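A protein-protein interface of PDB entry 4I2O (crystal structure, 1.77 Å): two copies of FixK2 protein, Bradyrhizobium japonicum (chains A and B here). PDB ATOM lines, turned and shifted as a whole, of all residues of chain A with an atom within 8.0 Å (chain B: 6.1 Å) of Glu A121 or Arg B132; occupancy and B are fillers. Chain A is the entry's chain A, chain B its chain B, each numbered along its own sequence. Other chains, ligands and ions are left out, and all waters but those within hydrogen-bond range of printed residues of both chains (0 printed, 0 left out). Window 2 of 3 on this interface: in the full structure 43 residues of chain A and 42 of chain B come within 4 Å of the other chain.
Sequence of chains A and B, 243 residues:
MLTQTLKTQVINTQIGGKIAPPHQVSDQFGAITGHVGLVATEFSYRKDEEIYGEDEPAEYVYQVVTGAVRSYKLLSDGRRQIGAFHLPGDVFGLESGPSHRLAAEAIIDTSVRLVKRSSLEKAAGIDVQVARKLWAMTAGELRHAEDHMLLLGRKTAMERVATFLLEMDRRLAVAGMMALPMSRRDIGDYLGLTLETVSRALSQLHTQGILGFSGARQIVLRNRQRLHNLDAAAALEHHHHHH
Of the printed residues of chain B, Leu A94 touches Trp B135.
Of chain B, only Arg B132 (3.7 Å) comes within 4 Å of Glu A121.
Ala A124 touches none of the printed residues of chain B.
Printed residues of chain B within 4 Å of Leu A134: Trp B135 (3.8 Å).
Arg B132 touches three residues of chain A.
Of the printed residues of chain A, Ala B136 touches Ser A96.
The nearest printed residue of chain B that does not touch Ser A96 is Met B137 (6.0 Å).
Among the printed residues, pairs that only touch across the chains: Arg A117 with Trp B135 (3.6 Å), Ser A96 with Ala B136 (3.7 Å), Trp A135 with Trp B135 (3.8 Å), Leu A134 with Trp B135 (3.8 Å), Trp A135 with Leu B134 (3.8 Å), Ser A96 with Trp B135 (3.9 Å) and Leu A94 with Trp B135 (3.9 Å).
O of Ser A96 lies within hydrogen-bond range of NH2 of Arg B132 (2.5 Å).
The side-chain carboxylate (OE2) of Glu A121 lies within salt-bridge range of the guanidinium group (NE) of Arg B132, at 3.7 Å.
NH2 of Arg B132 sits close to NH2 of Arg A117 (3.5 Å).
Hydrophobic or aromatic side chains of chain B that line the printed part of chain A: Trp B135 and Ala B136.
Hydrophobic or aromatic side chains of chain A within 4 Å of the printed part of chain B: Leu A94, Leu A134 and Trp A135.
Among the printed residues, Asp or Glu carboxylates within 4 Å of a Lys or Arg side-chain nitrogen of the other chain: Glu A121 with Arg B132 (3.7 Å).
Leu A134 touches Trp B135, and with the chains exchanged Trp A135 touches Leu B134.
Trp B135 touches its own counterpart, Trp A135.
5 positions are printed for both chains.
NH1 of Arg A117 is in salt-bridge range of OE1 of Glu A121.
O of Ser A96 sits at hydrogen-bond distance from NH2 of Arg A117, at 3.4 Å.
O of Glu A95 sits at hydrogen-bond distance from NE of Arg A117, 2.9 Å away.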
ATOM      1  N   VAL A  61      -5.317 -26.887  -7.651  1.00  0.00           N
ATOM      2  CA  VAL A  61      -5.601 -25.592  -8.273  1.00  0.00           C
ATOM      3  C   VAL A  61      -5.405 -24.577  -7.167  1.00  0.00           C
ATOM      4  O   VAL A  61      -5.678 -24.879  -6.012  1.00  0.00           O
ATOM      5  CB  VAL A  61      -7.031 -25.526  -8.814  1.00  0.00           C
ATOM      6  CG1 VAL A  61      -7.282 -24.209  -9.546  1.00  0.00           C
ATOM      7  CG2 VAL A  61      -7.263 -26.703  -9.803  1.00  0.00           C
ATOM      8  N   LEU A  94      -5.301 -24.362 -13.004  1.00  0.00           N
ATOM      9  CA  LEU A  94      -6.462 -25.130 -13.461  1.00  0.00           C
ATOM     10  C   LEU A  94      -6.183 -25.746 -14.831  1.00  0.00           C
ATOM     11  O   LEU A  94      -5.796 -25.038 -15.779  1.00  0.00           O
ATOM     12  CB  LEU A  94      -7.723 -24.246 -13.549  1.00  0.00           C
ATOM     13  CG  LEU A  94      -9.015 -24.983 -13.979  1.00  0.00           C
ATOM     14  CD1 LEU A  94      -9.479 -26.052 -12.979  1.00  0.00           C
ATOM     15  CD2 LEU A  94     -10.090 -23.932 -14.248  1.00  0.00           C
ATOM     16  N   GLU A  95      -6.339 -27.062 -14.916  1.00  0.00           N
ATOM     17  CA  GLU A  95      -6.159 -27.781 -16.182  1.00  0.00           C
ATOM     18  C   GLU A  95      -7.309 -28.708 -16.423  1.00  0.00           C
ATOM     19  O   GLU A  95      -7.825 -29.408 -15.489  1.00  0.00           O
ATOM     20  CB  GLU A  95      -4.834 -28.551 -16.211  1.00  0.00           C
ATOM     21  CG  GLU A  95      -3.591 -27.636 -16.050  1.00  0.00           C
ATOM     22  CD  GLU A  95      -3.057 -27.060 -17.375  1.00  0.00           C
ATOM     23  OE1 GLU A  95      -3.663 -27.316 -18.441  1.00  0.00           O
ATOM     24  OE2 GLU A  95      -2.032 -26.345 -17.339  1.00  0.00           O
ATOM     25  N   SER A  96      -7.755 -28.737 -17.687  1.00  0.00           N
ATOM     26  CA  SER A  96      -8.781 -29.665 -18.040  1.00  0.00           C
ATOM     27  C   SER A  96      -8.090 -31.014 -18.161  1.00  0.00           C
ATOM     28  O   SER A  96      -8.655 -32.059 -17.820  1.00  0.00           O
ATOM     29  CB  SER A  96      -9.374 -29.283 -19.393  1.00  0.00           C
ATOM     30  OG  SER A  96     -10.117 -30.357 -19.910  1.00  0.00           O
ATOM     31  N   GLY A  97      -6.866 -30.983 -18.676  1.00  0.00           N
ATOM     32  CA  GLY A  97      -6.125 -32.213 -18.896  1.00  0.00           C
ATOM     33  C   GLY A  97      -5.388 -32.626 -17.632  1.00  0.00           C
ATOM     34  O   GLY A  97      -5.612 -32.059 -16.551  1.00  0.00           O
ATOM     35  N   PRO A  98      -4.496 -33.615 -17.760  1.00  0.00           N
ATOM     36  CA  PRO A  98      -3.913 -34.314 -16.610  1.00  0.00           C
ATOM     37  C   PRO A  98      -2.649 -33.647 -16.062  1.00  0.00           C
ATOM     38  O   PRO A  98      -2.185 -34.031 -14.996  1.00  0.00           O
ATOM     39  CB  PRO A  98      -3.585 -35.700 -17.189  1.00  0.00           C
ATOM     40  CG  PRO A  98      -3.260 -35.422 -18.632  1.00  0.00           C
ATOM     41  CD  PRO A  98      -4.092 -34.217 -19.051  1.00  0.00           C
ATOM     42  N   LYS A 116      -8.019 -29.524  -4.049  1.00  0.00           N
ATOM     43  CA  LYS A 116      -7.686 -30.622  -4.940  1.00  0.00           C
ATOM     44  C   LYS A 116      -8.476 -30.486  -6.236  1.00  0.00           C
ATOM     45  O   LYS A 116      -9.671 -30.182  -6.221  1.00  0.00           O
ATOM     46  CB  LYS A 116      -7.970 -31.990  -4.337  1.00  0.00           C
ATOM     47  CG  LYS A 116      -7.218 -32.262  -3.071  1.00  0.00           C
ATOM     48  CD  LYS A 116      -7.265 -33.745  -2.698  1.00  0.00           C
ATOM     49  CE  LYS A 116      -6.647 -33.946  -1.315  1.00  0.00           C
ATOM     50  NZ  LYS A 116      -7.386 -33.176  -0.267  1.00  0.00           N
ATOM     51  N   ARG A 117      -7.777 -30.691  -7.339  1.00  0.00           N
ATOM     52  CA  ARG A 117      -8.414 -30.772  -8.646  1.00  0.00           C
ATOM     53  C   ARG A 117      -9.565 -31.805  -8.635  1.00  0.00           C
ATOM     54  O   ARG A 117     -10.639 -31.563  -9.193  1.00  0.00           O
ATOM     55  CB  ARG A 117      -7.359 -31.105  -9.692  1.00  0.00           C
ATOM     56  CG  ARG A 117      -7.882 -31.327 -11.098  1.00  0.00           C
ATOM     57  CD  ARG A 117      -8.645 -30.140 -11.669  1.00  0.00           C
ATOM     58  NE  ARG A 117      -8.998 -30.390 -13.076  1.00  0.00           N
ATOM     59  CZ  ARG A 117      -9.871 -31.321 -13.483  1.00  0.00           C
ATOM     60  NH1 ARG A 117     -10.476 -32.128 -12.610  1.00  0.00           N
ATOM     61  NH2 ARG A 117     -10.136 -31.466 -14.772  1.00  0.00           N
ATOM     62  N   SER A 118      -9.381 -32.932  -7.958  1.00  0.00           N
ATOM     63  CA  SER A 118     -10.440 -33.949  -7.942  1.00  0.00           C
ATOM     64  C   SER A 118     -11.671 -33.440  -7.179  1.00  0.00           C
ATOM     65  O   SER A 118     -12.810 -33.847  -7.433  1.00  0.00           O
ATOM     66  CB  SER A 118      -9.921 -35.242  -7.313  1.00  0.00           C
ATOM     67  OG  SER A 118      -9.340 -35.012  -6.033  1.00  0.00           O
ATOM     68  N   SER A 119     -11.440 -32.555  -6.218  1.00  0.00           N
ATOM     69  CA  SER A 119     -12.547 -31.962  -5.490  1.00  0.00           C
ATOM     70  C   SER A 119     -13.399 -31.059  -6.398  1.00  0.00           C
ATOM     71  O   SER A 119     -14.631 -31.067  -6.286  1.00  0.00           O
ATOM     72  CB  SER A 119     -12.036 -31.216  -4.254  1.00  0.00           C
ATOM     73  OG  SER A 119     -11.791 -32.174  -3.246  1.00  0.00           O
ATOM     74  N   LEU A 120     -12.738 -30.310  -7.287  1.00  0.00           N
ATOM     75  CA  LEU A 120     -13.406 -29.453  -8.280  1.00  0.00           C
ATOM     76  C   LEU A 120     -14.183 -30.271  -9.309  1.00  0.00           C
ATOM     77  O   LEU A 120     -15.308 -29.904  -9.692  1.00  0.00           O
ATOM     78  CB  LEU A 120     -12.389 -28.538  -9.015  1.00  0.00           C
ATOM     79  CG  LEU A 120     -11.897 -27.371  -8.157  1.00  0.00           C
ATOM     80  CD1 LEU A 120     -10.837 -26.553  -8.867  1.00  0.00           C
ATOM     81  CD2 LEU A 120     -13.051 -26.477  -7.738  1.00  0.00           C
ATOM     82  N   GLU A 121     -13.563 -31.353  -9.792  1.00  0.00           N
ATOM     83  CA  GLU A 121     -14.192 -32.262 -10.771  1.00  0.00           C
ATOM     84  C   GLU A 121     -15.488 -32.835 -10.194  1.00  0.00           C
ATOM     85  O   GLU A 121     -16.475 -33.031 -10.902  1.00  0.00           O
ATOM     86  CB  GLU A 121     -13.226 -33.402 -11.127  1.00  0.00           C
ATOM     87  CG  GLU A 121     -13.729 -34.399 -12.194  1.00  0.00           C
ATOM     88  CD  GLU A 121     -13.735 -33.827 -13.621  1.00  0.00           C
ATOM     89  OE1 GLU A 121     -12.924 -32.917 -13.908  1.00  0.00           O
ATOM     90  OE2 GLU A 121     -14.550 -34.299 -14.457  1.00  0.00           O
ATOM     91  N   LYS A 122     -15.497 -33.113  -8.902  1.00  0.00           N
ATOM     92  CA  LYS A 122     -16.709 -33.680  -8.301  1.00  0.00           C
ATOM     93  C   LYS A 122     -17.829 -32.636  -8.186  1.00  0.00           C
ATOM     94  O   LYS A 122     -19.002 -32.923  -8.499  1.00  0.00           O
ATOM     95  CB  LYS A 122     -16.435 -34.288  -6.938  1.00  0.00           C
ATOM     96  N   ALA A 123     -17.466 -31.429  -7.748  1.00  0.00           N
ATOM     97  CA  ALA A 123     -18.427 -30.326  -7.656  1.00  0.00           C
ATOM     98  C   ALA A 123     -19.004 -29.994  -9.041  1.00  0.00           C
ATOM     99  O   ALA A 123     -20.209 -29.752  -9.195  1.00  0.00           O
ATOM    100  CB  ALA A 123     -17.737 -29.077  -7.029  1.00  0.00           C
ATOM    101  N   ALA A 124     -18.143 -30.001 -10.060  1.00  0.00           N
ATOM    102  CA  ALA A 124     -18.586 -29.681 -11.410  1.00  0.00           C
ATOM    103  C   ALA A 124     -19.526 -30.729 -11.955  1.00  0.00           C
ATOM    104  O   ALA A 124     -20.331 -30.426 -12.827  1.00  0.00           O
ATOM    105  CB  ALA A 124     -17.376 -29.487 -12.376  1.00  0.00           C
ATOM    106  N   GLY A 125     -19.414 -31.959 -11.464  1.00  0.00           N
ATOM    107  CA  GLY A 125     -20.301 -33.020 -11.904  1.00  0.00           C
ATOM    108  C   GLY A 125     -21.639 -32.912 -11.213  1.00  0.00           C
ATOM    109  O   GLY A 125     -22.668 -33.371 -11.763  1.00  0.00           O
ATOM    110  N   ILE A 126     -21.621 -32.313 -10.022  1.00  0.00           N
ATOM    111  CA  ILE A 126     -22.806 -32.191  -9.188  1.00  0.00           C
ATOM    112  C   ILE A 126     -23.567 -30.930  -9.613  1.00  0.00           C
ATOM    113  O   ILE A 126     -24.798 -30.919  -9.675  1.00  0.00           O
ATOM    114  CB  ILE A 126     -22.421 -32.131  -7.672  1.00  0.00           C
ATOM    115  CG1 ILE A 126     -22.018 -33.524  -7.155  1.00  0.00           C
ATOM    116  CG2 ILE A 126     -23.562 -31.514  -6.836  1.00  0.00           C
ATOM    117  CD1 ILE A 126     -21.418 -33.524  -5.758  1.00  0.00           C
ATOM    118  N   ASP A 127     -22.834 -29.864  -9.908  1.00  0.00           N
ATOM    119  CA  ASP A 127     -23.467 -28.575 -10.208  1.00  0.00           C
ATOM    120  C   ASP A 127     -23.083 -28.001 -11.582  1.00  0.00           C
ATOM    121  O   ASP A 127     -21.927 -27.641 -11.807  1.00  0.00           O
ATOM    122  CB  ASP A 127     -23.138 -27.572  -9.099  1.00  0.00           C
ATOM    123  CG  ASP A 127     -23.878 -26.241  -9.256  1.00  0.00           C
ATOM    124  OD1 ASP A 127     -24.724 -26.093 -10.173  1.00  0.00           O
ATOM    125  OD2 ASP A 127     -23.616 -25.348  -8.432  1.00  0.00           O
ATOM    126  N   VAL A 130     -20.983 -24.763 -11.458  1.00  0.00           N
ATOM    127  CA  VAL A 130     -19.562 -24.988 -11.209  1.00  0.00           C
ATOM    128  C   VAL A 130     -18.839 -25.389 -12.517  1.00  0.00           C
ATOM    129  O   VAL A 130     -17.851 -24.751 -12.905  1.00  0.00           O
ATOM    130  CB  VAL A 130     -19.351 -26.037 -10.120  1.00  0.00           C
ATOM    131  CG1 VAL A 130     -17.872 -26.333 -10.013  1.00  0.00           C
ATOM    132  CG2 VAL A 130     -19.879 -25.519  -8.796  1.00  0.00           C
ATOM    133  N   ALA A 131     -19.332 -26.419 -13.220  1.00  0.00           N
ATOM    134  CA  ALA A 131     -18.754 -26.830 -14.517  1.00  0.00           C
ATOM    135  C   ALA A 131     -18.602 -25.650 -15.464  1.00  0.00           C
ATOM    136  O   ALA A 131     -17.591 -25.497 -16.184  1.00  0.00           O
ATOM    137  CB  ALA A 131     -19.647 -27.952 -15.160  1.00  0.00           C
ATOM    138  N   LEU A 134     -15.756 -23.298 -14.341  1.00  0.00           N
ATOM    139  CA  LEU A 134     -14.445 -23.865 -14.714  1.00  0.00           C
ATOM    140  C   LEU A 134     -14.108 -23.615 -16.186  1.00  0.00           C
ATOM    141  O   LEU A 134     -13.016 -23.137 -16.537  1.00  0.00           O
ATOM    142  CB  LEU A 134     -14.372 -25.358 -14.367  1.00  0.00           C
ATOM    143  CG  LEU A 134     -14.368 -25.700 -12.857  1.00  0.00           C
ATOM    144  CD1 LEU A 134     -14.442 -27.210 -12.704  1.00  0.00           C
ATOM    145  CD2 LEU A 134     -13.125 -25.070 -12.032  1.00  0.00           C
ATOM    146  N   TRP A 135     -15.063 -23.921 -17.063  1.00  0.00           N
ATOM    147  CA  TRP A 135     -14.903 -23.590 -18.492  1.00  0.00           C
ATOM    148  C   TRP A 135     -14.628 -22.097 -18.665  1.00  0.00           C
ATOM    149  O   TRP A 135     -13.695 -21.687 -19.378  1.00  0.00           O
ATOM    150  CB  TRP A 135     -16.193 -23.961 -19.216  1.00  0.00           C
ATOM    151  CG  TRP A 135     -16.104 -23.784 -20.696  1.00  0.00           C
ATOM    152  CD1 TRP A 135     -14.968 -23.614 -21.461  1.00  0.00           C
ATOM    153  CD2 TRP A 135     -17.214 -23.722 -21.585  1.00  0.00           C
ATOM    154  NE1 TRP A 135     -15.345 -23.499 -22.801  1.00  0.00           N
ATOM    155  CE2 TRP A 135     -16.717 -23.541 -22.884  1.00  0.00           C
ATOM    156  CE3 TRP A 135     -18.594 -23.791 -21.393  1.00  0.00           C
ATOM    157  CZ2 TRP A 135     -17.569 -23.452 -24.013  1.00  0.00           C
ATOM    158  CZ3 TRP A 135     -19.445 -23.692 -22.531  1.00  0.00           C
ATOM    159  CH2 TRP A 135     -18.915 -23.522 -23.801  1.00  0.00           C
ATOM    160  N   ASP B 127     -26.121 -32.902 -20.087  1.00  0.00           N
ATOM    161  CA  ASP B 127     -25.138 -33.988 -20.059  1.00  0.00           C
ATOM    162  C   ASP B 127     -23.772 -33.497 -19.568  1.00  0.00           C
ATOM    163  O   ASP B 127     -23.060 -32.763 -20.284  1.00  0.00           O
ATOM    164  CB  ASP B 127     -25.004 -34.594 -21.463  1.00  0.00           C
ATOM    165  CG  ASP B 127     -24.218 -35.914 -21.489  1.00  0.00           C
ATOM    166  OD1 ASP B 127     -23.678 -36.348 -20.443  1.00  0.00           O
ATOM    167  OD2 ASP B 127     -24.158 -36.531 -22.576  1.00  0.00           O
ATOM    168  N   VAL B 128     -23.405 -33.924 -18.362  1.00  0.00           N
ATOM    169  CA  VAL B 128     -22.076 -33.636 -17.803  1.00  0.00           C
ATOM    170  C   VAL B 128     -20.945 -33.956 -18.781  1.00  0.00           C
ATOM    171  O   VAL B 128     -19.919 -33.254 -18.789  1.00  0.00           O
ATOM    172  CB  VAL B 128     -21.828 -34.398 -16.458  1.00  0.00           C
ATOM    173  CG1 VAL B 128     -21.883 -35.896 -16.673  1.00  0.00           C
ATOM    174  CG2 VAL B 128     -20.473 -34.014 -15.839  1.00  0.00           C
ATOM    175  N   GLN B 129     -21.119 -34.983 -19.627  1.00  0.00           N
ATOM    176  CA  GLN B 129     -20.053 -35.362 -20.583  1.00  0.00           C
ATOM    177  C   GLN B 129     -19.867 -34.349 -21.722  1.00  0.00           C
ATOM    178  O   GLN B 129     -18.746 -34.152 -22.256  1.00  0.00           O
ATOM    179  CB  GLN B 129     -20.354 -36.740 -21.181  1.00  0.00           C
ATOM    180  CG  GLN B 129     -19.387 -37.865 -20.809  1.00  0.00           C
ATOM    181  N   VAL B 130     -20.973 -33.738 -22.134  1.00  0.00           N
ATOM    182  CA  VAL B 130     -20.935 -32.686 -23.139  1.00  0.00           C
ATOM    183  C   VAL B 130     -20.246 -31.451 -22.536  1.00  0.00           C
ATOM    184  O   VAL B 130     -19.332 -30.869 -23.148  1.00  0.00           O
ATOM    185  CB  VAL B 130     -22.341 -32.351 -23.644  1.00  0.00           C
ATOM    186  CG1 VAL B 130     -22.254 -31.146 -24.573  1.00  0.00           C
ATOM    187  CG2 VAL B 130     -22.931 -33.558 -24.359  1.00  0.00           C
ATOM    188  N   ALA B 131     -20.654 -31.058 -21.331  1.00  0.00           N
ATOM    189  CA  ALA B 131     -20.062 -29.897 -20.667  1.00  0.00           C
ATOM    190  C   ALA B 131     -18.553 -30.066 -20.535  1.00  0.00           C
ATOM    191  O   ALA B 131     -17.778 -29.150 -20.766  1.00  0.00           O
ATOM    192  CB  ALA B 131     -20.742 -29.687 -19.293  1.00  0.00           C
ATOM    193  N   ARG B 132     -18.132 -31.286 -20.249  1.00  0.00           N
ATOM    194  CA  ARG B 132     -16.726 -31.601 -20.044  1.00  0.00           C
ATOM    195  C   ARG B 132     -15.953 -31.610 -21.357  1.00  0.00           C
ATOM    196  O   ARG B 132     -14.748 -31.291 -21.443  1.00  0.00           O
ATOM    197  CB  ARG B 132     -16.658 -32.955 -19.322  1.00  0.00           C
ATOM    198  CG  ARG B 132     -15.273 -33.368 -18.945  1.00  0.00           C
ATOM    199  CD  ARG B 132     -14.769 -32.458 -17.828  1.00  0.00           C
ATOM    200  NE  ARG B 132     -13.370 -32.713 -17.531  1.00  0.00           N
ATOM    201  CZ  ARG B 132     -12.374 -32.266 -18.288  1.00  0.00           C
ATOM    202  NH1 ARG B 132     -12.636 -31.531 -19.382  1.00  0.00           N
ATOM    203  NH2 ARG B 132     -11.123 -32.545 -17.946  1.00  0.00           N
ATOM    204  N   LYS B 133     -16.647 -31.965 -22.425  1.00  0.00           N
ATOM    205  CA  LYS B 133     -16.035 -31.947 -23.758  1.00  0.00           C
ATOM    206  C   LYS B 133     -15.905 -30.517 -24.282  1.00  0.00           C
ATOM    207  O   LYS B 133     -14.919 -30.169 -24.910  1.00  0.00           O
ATOM    208  CB  LYS B 133     -16.879 -32.834 -24.691  1.00  0.00           C
ATOM    209  CG  LYS B 133     -16.416 -32.788 -26.135  1.00  0.00           C
ATOM    210  CD  LYS B 133     -14.985 -33.315 -26.320  1.00  0.00           C
ATOM    211  CE  LYS B 133     -14.679 -33.543 -27.816  1.00  0.00           C
ATOM    212  NZ  LYS B 133     -13.408 -34.292 -28.079  1.00  0.00           N
ATOM    213  N   LEU B 134     -16.888 -29.665 -24.021  1.00  0.00           N
ATOM    214  CA  LEU B 134     -16.701 -28.247 -24.364  1.00  0.00           C
ATOM    215  C   LEU B 134     -15.507 -27.625 -23.649  1.00  0.00           C
ATOM    216  O   LEU B 134     -14.664 -26.960 -24.264  1.00  0.00           O
ATOM    217  CB  LEU B 134     -17.964 -27.458 -24.058  1.00  0.00           C
ATOM    218  CG  LEU B 134     -19.136 -27.984 -24.879  1.00  0.00           C
ATOM    219  CD1 LEU B 134     -20.323 -27.225 -24.374  1.00  0.00           C
ATOM    220  CD2 LEU B 134     -18.920 -27.793 -26.466  1.00  0.00           C
ATOM    221  N   TRP B 135     -15.399 -27.872 -22.354  1.00  0.00           N
ATOM    222  CA  TRP B 135     -14.222 -27.310 -21.621  1.00  0.00           C
ATOM    223  C   TRP B 135     -12.939 -27.850 -22.220  1.00  0.00           C
ATOM    224  O   TRP B 135     -11.966 -27.113 -22.465  1.00  0.00           O
ATOM    225  CB  TRP B 135     -14.318 -27.773 -20.184  1.00  0.00           C
ATOM    226  CG  TRP B 135     -13.246 -27.258 -19.283  1.00  0.00           C
ATOM    227  CD1 TRP B 135     -12.403 -26.225 -19.497  1.00  0.00           C
ATOM    228  CD2 TRP B 135     -12.917 -27.810 -18.007  1.00  0.00           C
ATOM    229  NE1 TRP B 135     -11.559 -26.091 -18.384  1.00  0.00           N
ATOM    230  CE2 TRP B 135     -11.875 -27.063 -17.473  1.00  0.00           C
ATOM    231  CE3 TRP B 135     -13.434 -28.881 -17.262  1.00  0.00           C
ATOM    232  CZ2 TRP B 135     -11.331 -27.338 -16.196  1.00  0.00           C
ATOM    233  CZ3 TRP B 135     -12.890 -29.159 -16.013  1.00  0.00           C
ATOM    234  CH2 TRP B 135     -11.854 -28.392 -15.498  1.00  0.00           C
ATOM    235  N   ALA B 136     -12.902 -29.149 -22.481  1.00  0.00           N
ATOM    236  CA  ALA B 136     -11.720 -29.760 -23.139  1.00  0.00           C
ATOM    237  C   ALA B 136     -11.366 -29.119 -24.462  1.00  0.00           C
ATOM    238  O   ALA B 136     -10.173 -28.990 -24.793  1.00  0.00           O
ATOM    239  CB  ALA B 136     -11.928 -31.278 -23.318  1.00  0.00           C
ATOM    240  N   MET B 137     -12.374 -28.717 -25.245  1.00  0.00           N
ATOM    241  CA  MET B 137     -12.065 -28.072 -26.529  1.00  0.00           C
ATOM    242  C   MET B 137     -11.360 -26.736 -26.325  1.00  0.00           C
ATOM    243  O   MET B 137     -10.324 -26.444 -26.952  1.00  0.00           O
ATOM    244  CB  MET B 137     -13.351 -27.932 -27.371  1.00  0.00           C
ATOM    245  CG  MET B 137     -13.975 -29.295 -27.587  1.00  0.00           C
ATOM    246  SD  MET B 137     -15.558 -29.287 -28.485  1.00  0.00           S
ATOM    247  CE  MET B 137     -14.928 -28.307 -29.824  1.00  0.00           C
